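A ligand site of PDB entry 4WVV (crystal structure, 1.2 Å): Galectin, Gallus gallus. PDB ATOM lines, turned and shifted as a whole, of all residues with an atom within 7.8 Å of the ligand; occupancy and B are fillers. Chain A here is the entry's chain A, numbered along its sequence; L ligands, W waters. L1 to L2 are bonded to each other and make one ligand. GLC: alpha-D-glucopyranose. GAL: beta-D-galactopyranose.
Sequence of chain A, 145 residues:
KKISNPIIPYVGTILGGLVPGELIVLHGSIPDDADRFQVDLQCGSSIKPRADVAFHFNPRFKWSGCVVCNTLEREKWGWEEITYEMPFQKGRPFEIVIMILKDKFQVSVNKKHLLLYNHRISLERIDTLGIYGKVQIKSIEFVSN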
ATOM      1  N   ARG A  36      15.850  -0.018 -10.680  1.00  0.00           N
ATOM      2  CA  ARG A  36      14.615   0.693 -10.369  1.00  0.00           C
ATOM      3  C   ARG A  36      14.942   1.865  -9.462  1.00  0.00           C
ATOM      4  O   ARG A  36      16.019   1.899  -8.843  1.00  0.00           O
ATOM      5  CB  ARG A  36      13.616  -0.226  -9.669  1.00  0.00           C
ATOM      6  CG  ARG A  36      14.109  -0.806  -8.358  1.00  0.00           C
ATOM      7  CD  ARG A  36      12.991  -1.582  -7.684  1.00  0.00           C
ATOM      8  NE  ARG A  36      12.228  -0.755  -6.747  1.00  0.00           N
ATOM      9  CZ  ARG A  36      11.078  -1.146  -6.190  1.00  0.00           C
ATOM     10  NH1 ARG A  36      10.519  -2.285  -6.523  1.00  0.00           N
ATOM     11  NH2 ARG A  36      10.472  -0.361  -5.321  1.00  0.00           N
ATOM     12  N   PHE A  37      14.006   2.796  -9.359  1.00  0.00           N
ATOM     13  CA  PHE A  37      14.053   3.826  -8.339  1.00  0.00           C
ATOM     14  C   PHE A  37      12.622   4.192  -8.017  1.00  0.00           C
ATOM     15  O   PHE A  37      11.695   3.768  -8.711  1.00  0.00           O
ATOM     16  CB  PHE A  37      14.891   5.041  -8.791  1.00  0.00           C
ATOM     17  CG  PHE A  37      14.226   5.938  -9.827  1.00  0.00           C
ATOM     18  CD1 PHE A  37      13.521   7.068  -9.442  1.00  0.00           C
ATOM     19  CD2 PHE A  37      14.330   5.647 -11.178  1.00  0.00           C
ATOM     20  CE1 PHE A  37      12.932   7.880 -10.379  1.00  0.00           C
ATOM     21  CE2 PHE A  37      13.739   6.487 -12.123  1.00  0.00           C
ATOM     22  CZ  PHE A  37      13.045   7.603 -11.711  1.00  0.00           C
ATOM     23  N   GLN A  38      12.436   4.984  -6.958  1.00  0.00           N
ATOM     24  CA  GLN A  38      11.101   5.440  -6.636  1.00  0.00           C
ATOM     25  C   GLN A  38      11.084   6.851  -6.087  1.00  0.00           C
ATOM     26  O   GLN A  38      12.049   7.294  -5.444  1.00  0.00           O
ATOM     27  CB  GLN A  38      10.408   4.485  -5.677  1.00  0.00           C
ATOM     28  CG  GLN A  38      10.997   4.488  -4.281  1.00  0.00           C
ATOM     29  CD  GLN A  38      10.808   3.156  -3.571  1.00  0.00           C
ATOM     30  OE1 GLN A  38      11.308   2.132  -4.013  1.00  0.00           O
ATOM     31  NE2 GLN A  38      10.066   3.158  -2.485  1.00  0.00           N
ATOM     32  N   ASP A  40       8.460   8.836  -3.639  1.00  0.00           N
ATOM     33  CA  ASP A  40       7.376   8.575  -2.704  1.00  0.00           C
ATOM     34  C   ASP A  40       6.902   9.877  -2.059  1.00  0.00           C
ATOM     35  O   ASP A  40       7.696  10.622  -1.520  1.00  0.00           O
ATOM     36  CB  ASP A  40       7.868   7.613  -1.608  1.00  0.00           C
ATOM     37  CG  ASP A  40       8.127   6.202  -2.127  1.00  0.00           C
ATOM     38  OD1 ASP A  40       7.617   5.808  -3.199  1.00  0.00           O
ATOM     39  OD2 ASP A  40       8.856   5.461  -1.404  1.00  0.00           O
ATOM     40  N   ARG A  50       6.541   1.668   9.202  1.00  0.00           N
ATOM     41  CA  ARG A  50       6.871   2.414   7.995  1.00  0.00           C
ATOM     42  C   ARG A  50       5.811   3.456   7.651  1.00  0.00           C
ATOM     43  O   ARG A  50       4.619   3.142   7.609  1.00  0.00           O
ATOM     44  CB  ARG A  50       7.028   1.445   6.835  1.00  0.00           C
ATOM     45  CG  ARG A  50       7.427   2.146   5.575  1.00  0.00           C
ATOM     46  CD  ARG A  50       7.749   1.159   4.486  1.00  0.00           C
ATOM     47  NE  ARG A  50       7.946   1.845   3.211  1.00  0.00           N
ATOM     48  CZ  ARG A  50       8.060   1.205   2.057  1.00  0.00           C
ATOM     49  NH1 ARG A  50       8.020  -0.123   2.028  1.00  0.00           N
ATOM     50  NH2 ARG A  50       8.204   1.888   0.924  1.00  0.00           N
ATOM     51  N   HIS A  56       3.391   6.290  -4.529  1.00  0.00           N
ATOM     52  CA  HIS A  56       4.624   5.575  -4.826  1.00  0.00           C
ATOM     53  C   HIS A  56       4.714   5.496  -6.341  1.00  0.00           C
ATOM     54  O   HIS A  56       3.864   4.901  -6.960  1.00  0.00           O
ATOM     55  CB  HIS A  56       4.530   4.193  -4.198  1.00  0.00           C
ATOM     56  CG  HIS A  56       5.618   3.230  -4.580  1.00  0.00           C
ATOM     57  ND1 HIS A  56       6.917   3.348  -4.130  1.00  0.00           N
ATOM     58  CD2 HIS A  56       5.580   2.077  -5.295  1.00  0.00           C
ATOM     59  CE1 HIS A  56       7.609   2.300  -4.530  1.00  0.00           C
ATOM     60  NE2 HIS A  56       6.829   1.521  -5.254  1.00  0.00           N
ATOM     61  N   PHE A  57       5.742   6.143  -6.894  1.00  0.00           N
ATOM     62  CA  PHE A  57       5.996   6.196  -8.326  1.00  0.00           C
ATOM     63  C   PHE A  57       7.305   5.449  -8.576  1.00  0.00           C
ATOM     64  O   PHE A  57       8.359   5.899  -8.153  1.00  0.00           O
ATOM     65  CB  PHE A  57       6.100   7.665  -8.717  1.00  0.00           C
ATOM     66  CG  PHE A  57       6.537   7.917 -10.156  1.00  0.00           C
ATOM     67  CD1 PHE A  57       5.614   7.921 -11.174  1.00  0.00           C
ATOM     68  CD2 PHE A  57       7.864   8.147 -10.468  1.00  0.00           C
ATOM     69  CE1 PHE A  57       5.997   8.169 -12.470  1.00  0.00           C
ATOM     70  CE2 PHE A  57       8.259   8.389 -11.765  1.00  0.00           C
ATOM     71  CZ  PHE A  57       7.318   8.401 -12.774  1.00  0.00           C
ATOM     72  N   ASN A  58       7.223   4.300  -9.264  1.00  0.00           N
ATOM     73  CA  ASN A  58       8.332   3.340  -9.232  1.00  0.00           C
ATOM     74  C   ASN A  58       8.683   2.809 -10.627  1.00  0.00           C
ATOM     75  O   ASN A  58       8.206   1.748 -11.050  1.00  0.00           O
ATOM     76  CB  ASN A  58       7.933   2.184  -8.296  1.00  0.00           C
ATOM     77  CG  ASN A  58       8.962   1.073  -8.171  1.00  0.00           C
ATOM     78  OD1 ASN A  58       8.597  -0.078  -7.929  1.00  0.00           O
ATOM     79  ND2 ASN A  58      10.237   1.385  -8.272  1.00  0.00           N
ATOM     80  N   ARG A  60      10.721   0.768 -13.230  1.00  0.00           N
ATOM     81  CA  ARG A  60      11.441  -0.497 -13.166  1.00  0.00           C
ATOM     82  C   ARG A  60      11.976  -0.802 -14.547  1.00  0.00           C
ATOM     83  O   ARG A  60      11.227  -0.827 -15.510  1.00  0.00           O
ATOM     84  CB  ARG A  60      10.535  -1.646 -12.692  1.00  0.00           C
ATOM     85  CG  ARG A  60       9.954  -1.426 -11.338  1.00  0.00           C
ATOM     86  CD  ARG A  60       9.035  -2.559 -10.934  1.00  0.00           C
ATOM     87  NE  ARG A  60       8.454  -2.304  -9.614  1.00  0.00           N
ATOM     88  CZ  ARG A  60       7.656  -3.149  -8.976  1.00  0.00           C
ATOM     89  NH1 ARG A  60       7.331  -4.309  -9.542  1.00  0.00           N
ATOM     90  NH2 ARG A  60       7.196  -2.842  -7.774  1.00  0.00           N
ATOM     91  N   VAL A  68       5.420   1.299 -11.997  1.00  0.00           N
ATOM     92  CA  VAL A  68       4.417   0.840 -11.061  1.00  0.00           C
ATOM     93  C   VAL A  68       4.080   1.972 -10.109  1.00  0.00           C
ATOM     94  O   VAL A  68       4.978   2.586  -9.519  1.00  0.00           O
ATOM     95  CB  VAL A  68       4.946  -0.373 -10.252  1.00  0.00           C
ATOM     96  CG1 VAL A  68       3.945  -0.803  -9.183  1.00  0.00           C
ATOM     97  CG2 VAL A  68       5.250  -1.526 -11.189  1.00  0.00           C
ATOM     98  N   CYS A  69       2.792   2.236  -9.939  1.00  0.00           N
ATOM     99  CA  CYS A  69       2.314   3.184  -8.944  1.00  0.00           C
ATOM    100  C   CYS A  69       1.411   2.463  -7.948  1.00  0.00           C
ATOM    101  O   CYS A  69       0.669   1.557  -8.287  1.00  0.00           O
ATOM    102  CB  CYS A  69       1.561   4.340  -9.591  1.00  0.00           C
ATOM    103  SG  CYS A  69       2.566   5.363 -10.674  1.00  0.00           S
ATOM    104  N   ASN A  70       1.480   2.903  -6.699  1.00  0.00           N
ATOM    105  CA  ASN A  70       0.692   2.299  -5.635  1.00  0.00           C
ATOM    106  C   ASN A  70       0.680   3.234  -4.432  1.00  0.00           C
ATOM    107  O   ASN A  70       1.279   4.304  -4.447  1.00  0.00           O
ATOM    108  CB  ASN A  70       1.291   0.922  -5.264  1.00  0.00           C
ATOM    109  CG  ASN A  70       0.262  -0.084  -4.766  1.00  0.00           C
ATOM    110  OD1 ASN A  70      -0.831   0.270  -4.353  1.00  0.00           O
ATOM    111  ND2 ASN A  70       0.665  -1.352  -4.744  1.00  0.00           N
ATOM    112  N   THR A  71      -0.023   2.782  -3.401  1.00  0.00           N
ATOM    113  CA  THR A  71      -0.162   3.446  -2.126  1.00  0.00           C
ATOM    114  C   THR A  71       0.131   2.426  -1.022  1.00  0.00           C
ATOM    115  O   THR A  71      -0.321   1.265  -1.089  1.00  0.00           O
ATOM    116  CB  THR A  71      -1.586   3.985  -1.954  1.00  0.00           C
ATOM    117  OG1 THR A  71      -1.808   5.029  -2.915  1.00  0.00           O
ATOM    118  CG2 THR A  71      -1.884   4.495  -0.547  1.00  0.00           C
ATOM    119  N   LEU A  72       0.922   2.835  -0.038  1.00  0.00           N
ATOM    120  CA  LEU A  72       1.209   2.018   1.143  1.00  0.00           C
ATOM    121  C   LEU A  72       0.466   2.631   2.316  1.00  0.00           C
ATOM    122  O   LEU A  72       0.650   3.805   2.628  1.00  0.00           O
ATOM    123  CB  LEU A  72       2.699   2.004   1.450  1.00  0.00           C
ATOM    124  CG  LEU A  72       3.107   1.072   2.600  1.00  0.00           C
ATOM    125  CD1 LEU A  72       3.183  -0.363   2.138  1.00  0.00           C
ATOM    126  CD2 LEU A  72       4.443   1.506   3.146  1.00  0.00           C
ATOM    127  N   TRP A  77       0.530  -2.683   0.891  1.00  0.00           N
ATOM    128  CA  TRP A  77       0.384  -2.154  -0.449  1.00  0.00           C
ATOM    129  C   TRP A  77      -1.024  -2.377  -0.978  1.00  0.00           C
ATOM    130  O   TRP A  77      -1.632  -3.411  -0.719  1.00  0.00           O
ATOM    131  CB  TRP A  77       1.391  -2.802  -1.403  1.00  0.00           C
ATOM    132  CG  TRP A  77       2.814  -2.365  -1.175  1.00  0.00           C
ATOM    133  CD1 TRP A  77       3.826  -3.111  -0.671  1.00  0.00           C
ATOM    134  CD2 TRP A  77       3.355  -1.062  -1.423  1.00  0.00           C
ATOM    135  NE1 TRP A  77       4.973  -2.363  -0.616  1.00  0.00           N
ATOM    136  CE2 TRP A  77       4.707  -1.088  -1.061  1.00  0.00           C
ATOM    137  CE3 TRP A  77       2.831   0.128  -1.936  1.00  0.00           C
ATOM    138  CZ2 TRP A  77       5.551   0.025  -1.189  1.00  0.00           C
ATOM    139  CZ3 TRP A  77       3.665   1.224  -2.069  1.00  0.00           C
ATOM    140  CH2 TRP A  77       5.002   1.165  -1.688  1.00  0.00           C
ATOM    141  N   GLY A  78      -1.522  -1.417  -1.751  1.00  0.00           N
ATOM    142  CA  GLY A  78      -2.798  -1.545  -2.437  1.00  0.00           C
ATOM    143  C   GLY A  78      -2.669  -2.216  -3.789  1.00  0.00           C
ATOM    144  O   GLY A  78      -1.700  -2.920  -4.070  1.00  0.00           O
ATOM    145  N   TRP A  79      -3.660  -1.989  -4.639  1.00  0.00           N
ATOM    146  CA  TRP A  79      -3.649  -2.487  -5.995  1.00  0.00           C
ATOM    147  C   TRP A  79      -2.640  -1.698  -6.826  1.00  0.00           C
ATOM    148  O   TRP A  79      -2.682  -0.473  -6.852  1.00  0.00           O
ATOM    149  CB  TRP A  79      -5.038  -2.365  -6.641  1.00  0.00           C
ATOM    150  CG  TRP A  79      -6.124  -3.103  -5.918  1.00  0.00           C
ATOM    151  CD1 TRP A  79      -6.007  -4.236  -5.172  1.00  0.00           C
ATOM    152  CD2 TRP A  79      -7.517  -2.743  -5.875  1.00  0.00           C
ATOM    153  NE1 TRP A  79      -7.236  -4.613  -4.674  1.00  0.00           N
ATOM    154  CE2 TRP A  79      -8.174  -3.712  -5.086  1.00  0.00           C
ATOM    155  CE3 TRP A  79      -8.266  -1.701  -6.428  1.00  0.00           C
ATOM    156  CZ2 TRP A  79      -9.549  -3.671  -4.843  1.00  0.00           C
ATOM    157  CZ3 TRP A  79      -9.630  -1.656  -6.175  1.00  0.00           C
ATOM    158  CH2 TRP A  79     -10.258  -2.630  -5.387  1.00  0.00           C
ATOM    159  N   GLU A  80      -1.746  -2.388  -7.519  1.00  0.00           N
ATOM    160  CA  GLU A  80      -0.803  -1.717  -8.386  1.00  0.00           C
ATOM    161  C   GLU A  80      -1.498  -1.169  -9.615  1.00  0.00           C
ATOM    162  O   GLU A  80      -2.379  -1.802 -10.173  1.00  0.00           O
ATOM    163  CB  GLU A  80       0.282  -2.692  -8.838  1.00  0.00           C
ATOM    164  CG  GLU A  80       1.230  -3.058  -7.727  1.00  0.00           C
ATOM    165  CD  GLU A  80       2.374  -3.973  -8.136  1.00  0.00           C
ATOM    166  OE1 GLU A  80       2.285  -4.667  -9.177  1.00  0.00           O
ATOM    167  OE2 GLU A  80       3.373  -4.033  -7.379  1.00  0.00           O
ATOM    168  N   GLU A  81      -1.061   0.010 -10.043  1.00  0.00           N
ATOM    169  CA  GLU A  81      -1.434   0.558 -11.348  1.00  0.00           C
ATOM    170  C   GLU A  81      -0.165   0.619 -12.157  1.00  0.00           C
ATOM    171  O   GLU A  81       0.754   1.361 -11.831  1.00  0.00           O
ATOM    172  CB  GLU A  81      -2.041   1.946 -11.209  1.00  0.00           C
ATOM    173  CG  GLU A  81      -3.318   1.928 -10.374  1.00  0.00           C
ATOM    174  CD  GLU A  81      -3.981   3.278 -10.198  1.00  0.00           C
ATOM    175  OE1 GLU A  81      -3.794   4.168 -11.044  1.00  0.00           O
ATOM    176  OE2 GLU A  81      -4.705   3.449  -9.196  1.00  0.00           O
ATOM    177  N   ILE A  82      -0.076  -0.228 -13.170  1.00  0.00           N
ATOM    178  CA  ILE A  82       1.149  -0.380 -13.938  1.00  0.00           C
ATOM    179  C   ILE A  82       1.005   0.264 -15.313  1.00  0.00           C
ATOM    180  O   ILE A  82       0.087  -0.041 -16.062  1.00  0.00           O
ATOM    181  CB  ILE A  82       1.525  -1.870 -14.104  1.00  0.00           C
ATOM    182  CG1 ILE A  82       1.556  -2.547 -12.731  1.00  0.00           C
ATOM    183  CG2 ILE A  82       2.882  -1.994 -14.812  1.00  0.00           C
ATOM    184  CD1 ILE A  82       1.901  -4.025 -12.763  1.00  0.00           C
HETATM  185  C1  GLC L   1       4.404  -8.806  -6.144  1.00  0.00           C
HETATM  186  C2  GLC L   1       4.368  -7.564  -7.084  1.00  0.00           C
HETATM  187  C3  GLC L   1       5.544  -6.678  -6.879  1.00  0.00           C
HETATM  188  C4  GLC L   1       5.715  -6.328  -5.479  1.00  0.00           C
HETATM  189  C5  GLC L   1       5.882  -7.609  -4.646  1.00  0.00           C
HETATM  190  C6  GLC L   1       6.014  -7.394  -3.242  1.00  0.00           C
HETATM  191  O1  GLC L   1       5.312  -9.712  -6.661  1.00  0.00           O
HETATM  192  O2  GLC L   1       4.186  -7.998  -8.382  1.00  0.00           O
HETATM  193  O3  GLC L   1       5.447  -5.500  -7.766  1.00  0.00           O
HETATM  194  O4  GLC L   1       6.850  -5.472  -5.293  1.00  0.00           O
HETATM  195  O5  GLC L   1       4.691  -8.434  -4.835  1.00  0.00           O
HETATM  196  O6  GLC L   1       4.952  -6.670  -2.667  1.00  0.00           O
HETATM  197  C1  GAL L   2       6.692  -4.391  -4.455  1.00  0.00           C
HETATM  198  C2  GAL L   2       7.985  -3.744  -4.139  1.00  0.00           C
HETATM  199  C3  GAL L   2       7.775  -2.467  -3.427  1.00  0.00           C
HETATM  200  C4  GAL L   2       6.865  -1.553  -4.157  1.00  0.00           C
HETATM  201  C5  GAL L   2       5.570  -2.271  -4.433  1.00  0.00           C
HETATM  202  C6  GAL L   2       4.550  -1.455  -5.189  1.00  0.00           C
HETATM  203  O2  GAL L   2       8.759  -4.638  -3.346  1.00  0.00           O
HETATM  204  O3  GAL L   2       9.017  -1.787  -3.164  1.00  0.00           O
HETATM  205  O4  GAL L   2       7.477  -1.124  -5.375  1.00  0.00           O
HETATM  206  O5  GAL L   2       5.807  -3.442  -5.195  1.00  0.00           O
HETATM  207  O6  GAL L   2       3.362  -2.097  -5.438  1.00  0.00           O
HETATM  208  O   HOH W   1       8.579  -5.341  -0.590  1.00  0.00           O
HETATM  209  O   HOH W   2       9.985  -6.793  -4.399  1.00  0.00           O
HETATM  210  O   HOH W   3      10.254  -3.126  -1.018  1.00  0.00           O
HETATM  211  O   HOH W   4       5.891  -5.782  -0.316  1.00  0.00           O
HETATM  212  O   HOH W   5       9.186  -5.802  -6.886  1.00  0.00           O
HETATM  213  O   HOH W   6       5.865  -9.444  -9.896  1.00  0.00           O
HETATM  214  O   HOH W   7       9.315   0.390  -1.329  1.00  0.00           O
HETATM  215  O   HOH W   8       4.049  -6.086 -10.509  1.00  0.00           O
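An oxygen (O4) of GAL L2 sits at hydrogen-bond distance from the side-chain amide oxygen of Asn 58, 3.0 Å away. O4 of GAL L2 lies within hydrogen-bond range of NE2 of His 56, at 2.7 Å. O6 of GAL L2 is in hydrogen-bond range of ND2 of Asn 70, 2.9 Å away. NH2 of Arg 36 lies within hydrogen-bond range of O3 of GAL L2, 3.0 Å away. OE2 of Glu 80 is in hydrogen-bond range of O3 of GLC L1. An oxygen (O3) of GLC L1 lies within hydrogen-bond range of the guanidinium group of Arg 60 (2.8 Å).
The side-chain amide nitrogen (ND2) of Asn 58 sits at hydrogen-bond distance from the backbone carbonyl oxygen (O) of Phe 37 (2.8 Å). NH2 of Arg 36 lies close to OD1 of Asn 58, 3.2 Å away. O of Trp 79 sits close to OD1 of Asn 70. N of His 56 lies within hydrogen-bond range of O of Asn 70 (2.9 Å). NH2 of Arg 36 lies within hydrogen-bond range of OE1 of Gln 38. ND1 of His 56 is in hydrogen-bond range of OD1 of Asp 40, at 2.7 Å. The side-chain amide nitrogen (ND2) of Asn 70 is in hydrogen-bond range of the backbone carbonyl oxygen (O) of Gly 78 (2.9 Å). NE of Arg 60 lies within hydrogen-bond range of OD1 of Asn 58 (2.8 Å).
CZ2 of Trp 77 touches C4 of GAL L2, 3.6 Å away. Hydrophobic or aromatic side chains within 4 Å of the ligand: His 56 and Trp 77. Of the 20 residues printed, 7 come within 4 Å of the ligand. The nearest printed residue that does not touch the ligand is Val 68 (4.005 Å).
Water W7 lies within hydrogen-bond range of an oxygen (O3) of GAL L2 (2.9 Å), the guanidinium group (NH2) of Arg 50 (2.9 Å) and the side-chain amide nitrogen (NE2) of Gln 38 (3.1 Å). Water W8 lies within hydrogen-bond range of the side-chain carboxylate of Glu 80 and an oxygen (O2) of GLC L1.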
